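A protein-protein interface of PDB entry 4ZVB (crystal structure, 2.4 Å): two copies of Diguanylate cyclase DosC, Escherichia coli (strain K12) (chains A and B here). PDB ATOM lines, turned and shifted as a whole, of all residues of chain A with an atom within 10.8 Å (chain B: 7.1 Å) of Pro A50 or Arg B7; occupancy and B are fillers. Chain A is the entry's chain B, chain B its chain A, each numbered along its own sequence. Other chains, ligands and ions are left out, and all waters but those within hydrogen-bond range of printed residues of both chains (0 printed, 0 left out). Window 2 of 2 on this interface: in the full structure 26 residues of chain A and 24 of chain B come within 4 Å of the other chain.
The guanidinium group (NH1) of Arg B7 is in salt-bridge range of the side-chain carboxylate (OD2) of Asp A49 (3.2 Å).
OE2 of Glu B11 lies within salt-bridge range of NH1 of Arg A113 (2.8 Å).
The side-chain carboxylate (OE2) of Glu B11 is in salt-bridge range of the side-chain amino group (NZ) of Lys A117, 2.6 Å away.
NH1 of Arg B153 lies within salt-bridge range of OD2 of Asp A49 (3.6 Å).
Of the 23 printed residues of chain A, 6 touch a printed residue of chain B.
Printed residues of chain A that touch a printed residue of chain B: Asp A49, Pro A50, Glu A106, Ile A107, Arg A113 and Lys A117.
Printed residues of chain B that touch a printed residue of chain A: Arg B7, Glu B11, Ile B146 and Arg B153.
Hydrophobic or aromatic side chains of chain B within 4 Å of the printed part of chain A: Ile B146.
Among the printed residues, 8 pairs touch across the chains.
No position is printed for both chains.
Of the 8 pairs that touch across the chains among the printed residues, none has its exchanged pair printed and touching as well.
Pro A50 touches Arg B7 (CD to NH1, 3.3 Å).
Arg B153 touches Glu A106.
Arg B153 touches Ile A107 (NH2 to CD1, 3.8 Å).
NH1 of Arg A113 touches CD1 of Ile B146 (3.3 Å).
Printed residues of chain B within 4 Å of Pro A50: Arg B7 (3.3 Å).
Arg B7 touches two residues of chain A.
No residue of chain A comes within 4 Å of Lys B6.
No residue of chain A comes within 4 Å of Met B8.
No residue of chain A comes within 4 Å of Asp B10.
Glu B11 touches two residues of chain A.
Of the printed residues of chain B, Lys A117 touches Glu B11 (2.6 Å).
Of the printed residues of chain B, Arg A113 touches Glu B11 and Ile B146.
Of the printed residues of chain B, Asp A49 touches Arg B7 and Arg B153.
Arg A47 touches none of the printed residues of chain B.
The side-chain carboxylate of Asp A49 lies within hydrogen-bond range of the backbone NH of His A51.
The side-chain carboxylate (OD1) of Asp A49 is in hydrogen-bond range of the backbone NH (N) of Ala A52.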
ATOM      1  N   TYR A  43     -20.110  30.020 -11.298  1.00  0.00           N
ATOM      2  CA  TYR A  43     -19.236  30.957 -10.600  1.00  0.00           C
ATOM      3  C   TYR A  43     -19.671  31.198  -9.158  1.00  0.00           C
ATOM      4  O   TYR A  43     -18.843  31.199  -8.249  1.00  0.00           O
ATOM      5  CB  TYR A  43     -19.174  32.288 -11.350  1.00  0.00           C
ATOM      6  CG  TYR A  43     -18.036  33.177 -10.902  1.00  0.00           C
ATOM      7  CD1 TYR A  43     -16.770  33.049 -11.457  1.00  0.00           C
ATOM      8  CD2 TYR A  43     -18.226  34.142  -9.921  1.00  0.00           C
ATOM      9  CE1 TYR A  43     -15.724  33.857 -11.051  1.00  0.00           C
ATOM     10  CE2 TYR A  43     -17.187  34.956  -9.509  1.00  0.00           C
ATOM     11  CZ  TYR A  43     -15.938  34.809 -10.077  1.00  0.00           C
ATOM     12  OH  TYR A  43     -14.901  35.617  -9.669  1.00  0.00           O
ATOM     13  N   ARG A  44     -20.970  31.400  -8.952  1.00  0.00           N
ATOM     14  CA  ARG A  44     -21.488  31.710  -7.625  1.00  0.00           C
ATOM     15  C   ARG A  44     -21.292  30.560  -6.643  1.00  0.00           C
ATOM     16  O   ARG A  44     -20.881  30.771  -5.504  1.00  0.00           O
ATOM     17  CB  ARG A  44     -22.975  32.056  -7.706  1.00  0.00           C
ATOM     18  CG  ARG A  44     -23.585  32.468  -6.379  1.00  0.00           C
ATOM     19  CD  ARG A  44     -25.053  32.827  -6.534  1.00  0.00           C
ATOM     20  NE  ARG A  44     -25.850  31.660  -6.900  1.00  0.00           N
ATOM     21  CZ  ARG A  44     -26.324  30.777  -6.027  1.00  0.00           C
ATOM     22  NH1 ARG A  44     -26.077  30.921  -4.733  1.00  0.00           N
ATOM     23  NH2 ARG A  44     -27.039  29.742  -6.450  1.00  0.00           N
ATOM     24  N   ILE A  45     -21.590  29.345  -7.090  1.00  0.00           N
ATOM     25  CA  ILE A  45     -21.462  28.166  -6.243  1.00  0.00           C
ATOM     26  C   ILE A  45     -19.998  27.833  -5.951  1.00  0.00           C
ATOM     27  O   ILE A  45     -19.638  27.502  -4.821  1.00  0.00           O
ATOM     28  CB  ILE A  45     -22.155  26.951  -6.885  1.00  0.00           C
ATOM     29  CG1 ILE A  45     -23.657  27.213  -7.002  1.00  0.00           C
ATOM     30  CG2 ILE A  45     -21.897  25.690  -6.074  1.00  0.00           C
ATOM     31  CD1 ILE A  45     -24.419  26.114  -7.693  1.00  0.00           C
ATOM     32  N   VAL A  46     -19.159  27.939  -6.976  1.00  0.00           N
ATOM     33  CA  VAL A  46     -17.735  27.637  -6.849  1.00  0.00           C
ATOM     34  C   VAL A  46     -17.016  28.589  -5.892  1.00  0.00           C
ATOM     35  O   VAL A  46     -16.232  28.153  -5.047  1.00  0.00           O
ATOM     36  CB  VAL A  46     -17.036  27.670  -8.225  1.00  0.00           C
ATOM     37  CG1 VAL A  46     -15.537  27.880  -8.071  1.00  0.00           C
ATOM     38  CG2 VAL A  46     -17.327  26.390  -8.993  1.00  0.00           C
ATOM     39  N   ARG A  47     -17.299  29.882  -6.015  1.00  0.00           N
ATOM     40  CA  ARG A  47     -16.608  30.894  -5.221  1.00  0.00           C
ATOM     41  C   ARG A  47     -16.916  30.774  -3.729  1.00  0.00           C
ATOM     42  O   ARG A  47     -16.224  31.363  -2.901  1.00  0.00           O
ATOM     43  CB  ARG A  47     -16.966  32.299  -5.712  1.00  0.00           C
ATOM     44  CG  ARG A  47     -18.368  32.752  -5.344  1.00  0.00           C
ATOM     45  CD  ARG A  47     -18.628  34.170  -5.822  1.00  0.00           C
ATOM     46  NE  ARG A  47     -17.728  35.129  -5.186  1.00  0.00           N
ATOM     47  CZ  ARG A  47     -17.923  35.651  -3.980  1.00  0.00           C
ATOM     48  NH1 ARG A  47     -18.990  35.308  -3.271  1.00  0.00           N
ATOM     49  NH2 ARG A  47     -17.051  36.516  -3.481  1.00  0.00           N
ATOM     50  N   ILE A  48     -17.956  30.016  -3.392  1.00  0.00           N
ATOM     51  CA  ILE A  48     -18.292  29.749  -1.997  1.00  0.00           C
ATOM     52  C   ILE A  48     -17.127  29.056  -1.297  1.00  0.00           C
ATOM     53  O   ILE A  48     -16.768  29.404  -0.172  1.00  0.00           O
ATOM     54  CB  ILE A  48     -19.558  28.876  -1.876  1.00  0.00           C
ATOM     55  CG1 ILE A  48     -20.779  29.627  -2.413  1.00  0.00           C
ATOM     56  CG2 ILE A  48     -19.788  28.450  -0.435  1.00  0.00           C
ATOM     57  CD1 ILE A  48     -22.041  28.794  -2.449  1.00  0.00           C
ATOM     58  N   ASP A  49     -16.536  28.077  -1.975  1.00  0.00           N
ATOM     59  CA  ASP A  49     -15.358  27.390  -1.461  1.00  0.00           C
ATOM     60  C   ASP A  49     -14.161  28.340  -1.403  1.00  0.00           C
ATOM     61  O   ASP A  49     -13.770  28.911  -2.422  1.00  0.00           O
ATOM     62  CB  ASP A  49     -15.035  26.170  -2.327  1.00  0.00           C
ATOM     63  CG  ASP A  49     -13.901  25.338  -1.764  1.00  0.00           C
ATOM     64  OD1 ASP A  49     -12.728  25.669  -2.032  1.00  0.00           O
ATOM     65  OD2 ASP A  49     -14.184  24.348  -1.056  1.00  0.00           O
ATOM     66  N   PRO A  50     -13.581  28.515  -0.205  1.00  0.00           N
ATOM     67  CA  PRO A  50     -12.443  29.414   0.029  1.00  0.00           C
ATOM     68  C   PRO A  50     -11.227  29.081  -0.831  1.00  0.00           C
ATOM     69  O   PRO A  50     -10.550  29.988  -1.316  1.00  0.00           O
ATOM     70  CB  PRO A  50     -12.128  29.200   1.513  1.00  0.00           C
ATOM     71  CG  PRO A  50     -13.406  28.727   2.105  1.00  0.00           C
ATOM     72  CD  PRO A  50     -14.043  27.884   1.043  1.00  0.00           C
ATOM     73  N   HIS A  51     -10.959  27.792  -1.013  1.00  0.00           N
ATOM     74  CA  HIS A  51      -9.794  27.346  -1.769  1.00  0.00           C
ATOM     75  C   HIS A  51      -9.927  27.694  -3.250  1.00  0.00           C
ATOM     76  O   HIS A  51      -8.930  27.829  -3.958  1.00  0.00           O
ATOM     77  CB  HIS A  51      -9.595  25.837  -1.598  1.00  0.00           C
ATOM     78  CG  HIS A  51      -8.190  25.379  -1.832  1.00  0.00           C
ATOM     79  ND1 HIS A  51      -7.449  25.772  -2.926  1.00  0.00           N
ATOM     80  CD2 HIS A  51      -7.392  24.553  -1.115  1.00  0.00           C
ATOM     81  CE1 HIS A  51      -6.255  25.212  -2.870  1.00  0.00           C
ATOM     82  NE2 HIS A  51      -6.193  24.467  -1.781  1.00  0.00           N
ATOM     83  N   ALA A  52     -11.165  27.837  -3.711  1.00  0.00           N
ATOM     84  CA  ALA A  52     -11.430  28.159  -5.109  1.00  0.00           C
ATOM     85  C   ALA A  52     -11.573  29.665  -5.313  1.00  0.00           C
ATOM     86  O   ALA A  52     -11.251  30.189  -6.379  1.00  0.00           O
ATOM     87  CB  ALA A  52     -12.680  27.439  -5.590  1.00  0.00           C
ATOM     88  N   GLU A  53     -12.062  30.351  -4.284  1.00  0.00           N
ATOM     89  CA  GLU A  53     -12.322  31.786  -4.358  1.00  0.00           C
ATOM     90  C   GLU A  53     -11.036  32.588  -4.543  1.00  0.00           C
ATOM     91  O   GLU A  53     -11.046  33.660  -5.149  1.00  0.00           O
ATOM     92  CB  GLU A  53     -13.062  32.255  -3.101  1.00  0.00           C
ATOM     93  CG  GLU A  53     -13.870  33.538  -3.271  1.00  0.00           C
ATOM     94  CD  GLU A  53     -13.020  34.791  -3.197  1.00  0.00           C
ATOM     95  OE1 GLU A  53     -11.975  34.764  -2.513  1.00  0.00           O
ATOM     96  OE2 GLU A  53     -13.398  35.803  -3.822  1.00  0.00           O
ATOM     97  N   GLU A  54      -9.929  32.059  -4.030  1.00  0.00           N
ATOM     98  CA  GLU A  54      -8.647  32.756  -4.087  1.00  0.00           C
ATOM     99  C   GLU A  54      -8.156  32.938  -5.520  1.00  0.00           C
ATOM    100  O   GLU A  54      -7.343  33.819  -5.797  1.00  0.00           O
ATOM    101  CB  GLU A  54      -7.593  32.010  -3.266  1.00  0.00           C
ATOM    102  CG  GLU A  54      -7.287  30.608  -3.762  1.00  0.00           C
ATOM    103  CD  GLU A  54      -6.348  29.857  -2.838  1.00  0.00           C
ATOM    104  OE1 GLU A  54      -5.876  30.459  -1.850  1.00  0.00           O
ATOM    105  OE2 GLU A  54      -6.077  28.667  -3.102  1.00  0.00           O
ATOM    106  N   PHE A  55      -8.658  32.107  -6.429  1.00  0.00           N
ATOM    107  CA  PHE A  55      -8.303  32.217  -7.838  1.00  0.00           C
ATOM    108  C   PHE A  55      -9.313  33.090  -8.573  1.00  0.00           C
ATOM    109  O   PHE A  55      -9.029  33.615  -9.649  1.00  0.00           O
ATOM    110  CB  PHE A  55      -8.234  30.837  -8.493  1.00  0.00           C
ATOM    111  CG  PHE A  55      -7.237  29.909  -7.860  1.00  0.00           C
ATOM    112  CD1 PHE A  55      -5.893  29.990  -8.186  1.00  0.00           C
ATOM    113  CD2 PHE A  55      -7.644  28.949  -6.950  1.00  0.00           C
ATOM    114  CE1 PHE A  55      -4.974  29.133  -7.611  1.00  0.00           C
ATOM    115  CE2 PHE A  55      -6.730  28.090  -6.369  1.00  0.00           C
ATOM    116  CZ  PHE A  55      -5.393  28.183  -6.700  1.00  0.00           C
ATOM    117  N   LEU A  56     -10.494  33.237  -7.983  1.00  0.00           N
ATOM    118  CA  LEU A  56     -11.564  34.023  -8.586  1.00  0.00           C
ATOM    119  C   LEU A  56     -11.877  35.261  -7.751  1.00  0.00           C
ATOM    120  O   LEU A  56     -12.977  35.391  -7.212  1.00  0.00           O
ATOM    121  CB  LEU A  56     -12.820  33.167  -8.751  1.00  0.00           C
ATOM    122  CG  LEU A  56     -12.612  31.813  -9.432  1.00  0.00           C
ATOM    123  CD1 LEU A  56     -13.929  31.064  -9.565  1.00  0.00           C
ATOM    124  CD2 LEU A  56     -11.949  31.989 -10.789  1.00  0.00           C
ATOM    125  N   SER A  57     -10.910  36.168  -7.649  1.00  0.00           N
ATOM    126  CA  SER A  57     -11.065  37.343  -6.798  1.00  0.00           C
ATOM    127  C   SER A  57     -11.552  38.562  -7.576  1.00  0.00           C
ATOM    128  O   SER A  57     -12.582  39.146  -7.242  1.00  0.00           O
ATOM    129  CB  SER A  57      -9.743  37.667  -6.099  1.00  0.00           C
ATOM    130  OG  SER A  57      -9.360  36.620  -5.225  1.00  0.00           O
ATOM    131  N   ILE A 103      -3.734  25.850 -10.063  1.00  0.00           N
ATOM    132  CA  ILE A 103      -5.002  25.386  -9.517  1.00  0.00           C
ATOM    133  C   ILE A 103      -4.967  23.887  -9.246  1.00  0.00           C
ATOM    134  O   ILE A 103      -4.728  23.093 -10.156  1.00  0.00           O
ATOM    135  CB  ILE A 103      -6.168  25.703 -10.469  1.00  0.00           C
ATOM    136  CG1 ILE A 103      -6.162  27.188 -10.834  1.00  0.00           C
ATOM    137  CG2 ILE A 103      -7.494  25.306  -9.839  1.00  0.00           C
ATOM    138  CD1 ILE A 103      -7.111  27.545 -11.952  1.00  0.00           C
ATOM    139  N   PRO A 104      -5.198  23.499  -7.982  1.00  0.00           N
ATOM    140  CA  PRO A 104      -5.190  22.100  -7.539  1.00  0.00           C
ATOM    141  C   PRO A 104      -6.173  21.231  -8.317  1.00  0.00           C
ATOM    142  O   PRO A 104      -7.204  21.724  -8.775  1.00  0.00           O
ATOM    143  CB  PRO A 104      -5.596  22.197  -6.067  1.00  0.00           C
ATOM    144  CG  PRO A 104      -5.192  23.566  -5.658  1.00  0.00           C
ATOM    145  CD  PRO A 104      -5.431  24.426  -6.862  1.00  0.00           C
ATOM    146  N   GLU A 106      -8.013  18.691  -7.233  1.00  0.00           N
ATOM    147  CA  GLU A 106      -9.235  18.436  -6.476  1.00  0.00           C
ATOM    148  C   GLU A 106     -10.206  19.611  -6.562  1.00  0.00           C
ATOM    149  O   GLU A 106     -11.413  19.444  -6.388  1.00  0.00           O
ATOM    150  CB  GLU A 106      -8.909  18.134  -5.009  1.00  0.00           C
ATOM    151  CG  GLU A 106      -8.258  19.280  -4.245  1.00  0.00           C
ATOM    152  CD  GLU A 106      -6.759  19.365  -4.466  1.00  0.00           C
ATOM    153  OE1 GLU A 106      -6.228  18.589  -5.289  1.00  0.00           O
ATOM    154  OE2 GLU A 106      -6.109  20.211  -3.815  1.00  0.00           O
ATOM    155  N   ILE A 107      -9.672  20.797  -6.834  1.00  0.00           N
ATOM    156  CA  ILE A 107     -10.489  21.997  -6.967  1.00  0.00           C
ATOM    157  C   ILE A 107     -11.188  22.029  -8.322  1.00  0.00           C
ATOM    158  O   ILE A 107     -12.365  22.378  -8.418  1.00  0.00           O
ATOM    159  CB  ILE A 107      -9.642  23.274  -6.790  1.00  0.00           C
ATOM    160  CG1 ILE A 107      -8.981  23.282  -5.411  1.00  0.00           C
ATOM    161  CG2 ILE A 107     -10.497  24.516  -6.967  1.00  0.00           C
ATOM    162  CD1 ILE A 107      -9.964  23.196  -4.261  1.00  0.00           C
ATOM    163  N   MET A 110     -13.931  19.572  -8.440  1.00  0.00           N
ATOM    164  CA  MET A 110     -15.045  20.103  -7.665  1.00  0.00           C
ATOM    165  C   MET A 110     -15.935  20.963  -8.555  1.00  0.00           C
ATOM    166  O   MET A 110     -17.153  21.001  -8.387  1.00  0.00           O
ATOM    167  CB  MET A 110     -14.529  20.907  -6.466  1.00  0.00           C
ATOM    168  CG  MET A 110     -15.611  21.571  -5.627  1.00  0.00           C
ATOM    169  SD  MET A 110     -15.956  23.268  -6.126  1.00  0.00           S
ATOM    170  CE  MET A 110     -14.344  24.019  -5.908  1.00  0.00           C
ATOM    171  N   ARG A 113     -18.153  18.699 -10.711  1.00  0.00           N
ATOM    172  CA  ARG A 113     -19.301  18.197  -9.964  1.00  0.00           C
ATOM    173  C   ARG A 113     -20.401  19.246  -9.894  1.00  0.00           C
ATOM    174  O   ARG A 113     -21.583  18.934 -10.044  1.00  0.00           O
ATOM    175  CB  ARG A 113     -18.891  17.782  -8.551  1.00  0.00           C
ATOM    176  CG  ARG A 113     -20.004  17.101  -7.774  1.00  0.00           C
ATOM    177  CD  ARG A 113     -19.524  16.621  -6.419  1.00  0.00           C
ATOM    178  NE  ARG A 113     -19.150  17.739  -5.560  1.00  0.00           N
ATOM    179  CZ  ARG A 113     -19.975  18.328  -4.701  1.00  0.00           C
ATOM    180  NH1 ARG A 113     -21.226  17.907  -4.586  1.00  0.00           N
ATOM    181  NH2 ARG A 113     -19.548  19.340  -3.959  1.00  0.00           N
ATOM    182  N   VAL A 114     -20.001  20.492  -9.657  1.00  0.00           N
ATOM    183  CA  VAL A 114     -20.933  21.612  -9.629  1.00  0.00           C
ATOM    184  C   VAL A 114     -21.609  21.775 -10.984  1.00  0.00           C
ATOM    185  O   VAL A 114     -22.822  21.975 -11.065  1.00  0.00           O
ATOM    186  CB  VAL A 114     -20.220  22.927  -9.243  1.00  0.00           C
ATOM    187  CG1 VAL A 114     -21.122  24.126  -9.499  1.00  0.00           C
ATOM    188  CG2 VAL A 114     -19.783  22.883  -7.786  1.00  0.00           C
ATOM    189  N   LYS A 117     -24.054  19.114 -11.579  1.00  0.00           N
ATOM    190  CA  LYS A 117     -25.160  19.296 -10.647  1.00  0.00           C
ATOM    191  C   LYS A 117     -26.163  20.342 -11.133  1.00  0.00           C
ATOM    192  O   LYS A 117     -27.372  20.122 -11.085  1.00  0.00           O
ATOM    193  CB  LYS A 117     -24.616  19.687  -9.271  1.00  0.00           C
ATOM    194  CG  LYS A 117     -25.605  19.546  -8.128  1.00  0.00           C
ATOM    195  CD  LYS A 117     -24.897  19.713  -6.791  1.00  0.00           C
ATOM    196  CE  LYS A 117     -25.828  19.432  -5.626  1.00  0.00           C
ATOM    197  NZ  LYS A 117     -25.167  19.719  -4.322  1.00  0.00           N
ATOM    198  N   PHE B   5     -15.925  20.094   6.383  1.00  0.00           N
ATOM    199  CA  PHE B   5     -16.824  18.991   6.699  1.00  0.00           C
ATOM    200  C   PHE B   5     -18.264  19.458   6.869  1.00  0.00           C
ATOM    201  O   PHE B   5     -19.195  18.805   6.397  1.00  0.00           O
ATOM    202  CB  PHE B   5     -16.368  18.272   7.971  1.00  0.00           C
ATOM    203  CG  PHE B   5     -17.450  17.462   8.629  1.00  0.00           C
ATOM    204  CD1 PHE B   5     -17.824  16.231   8.115  1.00  0.00           C
ATOM    205  CD2 PHE B   5     -18.098  17.934   9.759  1.00  0.00           C
ATOM    206  CE1 PHE B   5     -18.822  15.486   8.717  1.00  0.00           C
ATOM    207  CE2 PHE B   5     -19.097  17.194  10.365  1.00  0.00           C
ATOM    208  CZ  PHE B   5     -19.459  15.968   9.843  1.00  0.00           C
ATOM    209  N   LYS B   6     -18.435  20.583   7.559  1.00  0.00           N
ATOM    210  CA  LYS B   6     -19.761  21.119   7.843  1.00  0.00           C
ATOM    211  C   LYS B   6     -20.500  21.416   6.541  1.00  0.00           C
ATOM    212  O   LYS B   6     -21.686  21.120   6.403  1.00  0.00           O
ATOM    213  CB  LYS B   6     -19.654  22.381   8.702  1.00  0.00           C
ATOM    214  CG  LYS B   6     -20.987  23.016   9.062  1.00  0.00           C
ATOM    215  CD  LYS B   6     -21.889  22.022   9.777  1.00  0.00           C
ATOM    216  CE  LYS B   6     -23.226  22.638  10.151  1.00  0.00           C
ATOM    217  NZ  LYS B   6     -24.174  21.618  10.683  1.00  0.00           N
ATOM    218  N   ARG B   7     -19.782  21.996   5.585  1.00  0.00           N
ATOM    219  CA  ARG B   7     -20.345  22.316   4.280  1.00  0.00           C
ATOM    220  C   ARG B   7     -20.633  21.060   3.462  1.00  0.00           C
ATOM    221  O   ARG B   7     -21.613  21.005   2.717  1.00  0.00           O
ATOM    222  CB  ARG B   7     -19.389  23.232   3.516  1.00  0.00           C
ATOM    223  CG  ARG B   7     -19.862  23.650   2.139  1.00  0.00           C
ATOM    224  CD  ARG B   7     -18.762  24.407   1.423  1.00  0.00           C
ATOM    225  NE  ARG B   7     -18.231  25.486   2.250  1.00  0.00           N
ATOM    226  CZ  ARG B   7     -16.980  25.927   2.189  1.00  0.00           C
ATOM    227  NH1 ARG B   7     -16.122  25.377   1.340  1.00  0.00           N
ATOM    228  NH2 ARG B   7     -16.583  26.914   2.981  1.00  0.00           N
ATOM    229  N   MET B   8     -19.778  20.052   3.608  1.00  0.00           N
ATOM    230  CA  MET B   8     -19.959  18.783   2.908  1.00  0.00           C
ATOM    231  C   MET B   8     -21.129  17.991   3.476  1.00  0.00           C
ATOM    232  O   MET B   8     -21.877  17.351   2.737  1.00  0.00           O
ATOM    233  CB  MET B   8     -18.679  17.946   2.973  1.00  0.00           C
ATOM    234  CG  MET B   8     -17.496  18.537   2.219  1.00  0.00           C
ATOM    235  SD  MET B   8     -17.771  18.653   0.437  1.00  0.00           S
ATOM    236  CE  MET B   8     -18.204  20.383   0.256  1.00  0.00           C
ATOM    237  N   LYS B   9     -21.276  18.036   4.795  1.00  0.00           N
ATOM    238  CA  LYS B   9     -22.368  17.349   5.469  1.00  0.00           C
ATOM    239  C   LYS B   9     -23.706  17.946   5.052  1.00  0.00           C
ATOM    240  O   LYS B   9     -24.649  17.219   4.747  1.00  0.00           O
ATOM    241  CB  LYS B   9     -22.197  17.416   6.989  1.00  0.00           C
ATOM    242  CG  LYS B   9     -23.330  16.764   7.768  1.00  0.00           C
ATOM    243  CD  LYS B   9     -23.197  17.017   9.260  1.00  0.00           C
ATOM    244  CE  LYS B   9     -23.577  18.442   9.617  1.00  0.00           C
ATOM    245  NZ  LYS B   9     -24.957  18.776   9.169  1.00  0.00           N
ATOM    246  N   ASP B  10     -23.776  19.275   5.035  1.00  0.00           N
ATOM    247  CA  ASP B  10     -25.002  19.980   4.675  1.00  0.00           C
ATOM    248  C   ASP B  10     -25.430  19.692   3.239  1.00  0.00           C
ATOM    249  O   ASP B  10     -26.620  19.547   2.958  1.00  0.00           O
ATOM    250  CB  ASP B  10     -24.825  21.489   4.864  1.00  0.00           C
ATOM    251  CG  ASP B  10     -24.653  21.881   6.319  1.00  0.00           C
ATOM    252  OD1 ASP B  10     -25.104  21.120   7.201  1.00  0.00           O
ATOM    253  OD2 ASP B  10     -24.064  22.951   6.580  1.00  0.00           O
ATOM    254  N   GLU B  11     -24.461  19.610   2.332  1.00  0.00           N
ATOM    255  CA  GLU B  11     -24.760  19.383   0.922  1.00  0.00           C
ATOM    256  C   GLU B  11     -25.235  17.957   0.664  1.00  0.00           C
ATOM    257  O   GLU B  11     -26.165  17.736  -0.112  1.00  0.00           O
ATOM    258  CB  GLU B  11     -23.535  19.684   0.058  1.00  0.00           C
ATOM    259  CG  GLU B  11     -23.815  19.635  -1.435  1.00  0.00           C
ATOM    260  CD  GLU B  11     -22.598  19.965  -2.270  1.00  0.00           C
ATOM    261  OE1 GLU B  11     -21.504  20.135  -1.690  1.00  0.00           O
ATOM    262  OE2 GLU B  11     -22.732  20.051  -3.509  1.00  0.00           O
ATOM    263  N   TRP B  12     -24.595  16.994   1.319  1.00  0.00           N
ATOM    264  CA  TRP B  12     -24.968  15.593   1.168  1.00  0.00           C
ATOM    265  C   TRP B  12     -26.311  15.343   1.848  1.00  0.00           C
ATOM    266  O   TRP B  12     -27.140  14.582   1.348  1.00  0.00           O
ATOM    267  CB  TRP B  12     -23.883  14.680   1.745  1.00  0.00           C
ATOM    268  CG  TRP B  12     -23.889  13.294   1.169  1.00  0.00           C
ATOM    269  CD1 TRP B  12     -24.925  12.673   0.533  1.00  0.00           C
ATOM    270  CD2 TRP B  12     -22.797  12.367   1.157  1.00  0.00           C
ATOM    271  NE1 TRP B  12     -24.550  11.412   0.137  1.00  0.00           N
ATOM    272  CE2 TRP B  12     -23.247  11.200   0.506  1.00  0.00           C
ATOM    273  CE3 TRP B  12     -21.485  12.407   1.637  1.00  0.00           C
ATOM    274  CZ2 TRP B  12     -22.433  10.085   0.324  1.00  0.00           C
ATOM    275  CZ3 TRP B  12     -20.676  11.299   1.454  1.00  0.00           C
ATOM    276  CH2 TRP B  12     -21.154  10.153   0.803  1.00  0.00           C
ATOM    277  N   THR B  13     -26.517  15.992   2.990  1.00  0.00           N
ATOM    278  CA  THR B  13     -27.794  15.933   3.690  1.00  0.00           C
ATOM    279  C   THR B  13     -28.892  16.536   2.824  1.00  0.00           C
ATOM    280  O   THR B  13     -29.980  15.973   2.700  1.00  0.00           O
ATOM    281  CB  THR B  13     -27.740  16.679   5.039  1.00  0.00           C
ATOM    282  OG1 THR B  13     -26.807  16.028   5.910  1.00  0.00           O
ATOM    283  CG2 THR B  13     -29.109  16.701   5.697  1.00  0.00           C
ATOM    284  N   ILE B 146     -20.416  13.312  -4.931  1.00  0.00           N
ATOM    285  CA  ILE B 146     -20.078  13.928  -3.651  1.00  0.00           C
ATOM    286  C   ILE B 146     -19.209  12.976  -2.828  1.00  0.00           C
ATOM    287  O   ILE B 146     -18.328  13.411  -2.090  1.00  0.00           O
ATOM    288  CB  ILE B 146     -21.345  14.340  -2.850  1.00  0.00           C
ATOM    289  CG1 ILE B 146     -20.959  15.085  -1.570  1.00  0.00           C
ATOM    290  CG2 ILE B 146     -22.214  13.140  -2.519  1.00  0.00           C
ATOM    291  CD1 ILE B 146     -20.227  16.384  -1.812  1.00  0.00           C
ATOM    292  N   ARG B 153     -10.383  14.455  -1.712  1.00  0.00           N
ATOM    293  CA  ARG B 153      -9.857  15.576  -0.938  1.00  0.00           C
ATOM    294  C   ARG B 153      -9.388  15.158   0.455  1.00  0.00           C
ATOM    295  O   ARG B 153      -8.832  15.967   1.196  1.00  0.00           O
ATOM    296  CB  ARG B 153     -10.912  16.682  -0.832  1.00  0.00           C
ATOM    297  CG  ARG B 153     -11.346  17.230  -2.186  1.00  0.00           C
ATOM    298  CD  ARG B 153     -12.306  18.403  -2.058  1.00  0.00           C
ATOM    299  NE  ARG B 153     -11.651  19.606  -1.554  1.00  0.00           N
ATOM    300  CZ  ARG B 153     -12.211  20.811  -1.547  1.00  0.00           C
ATOM    301  NH1 ARG B 153     -13.438  20.977  -2.020  1.00  0.00           N
ATOM    302  NH2 ARG B 153     -11.542  21.852  -1.071  1.00  0.00           N
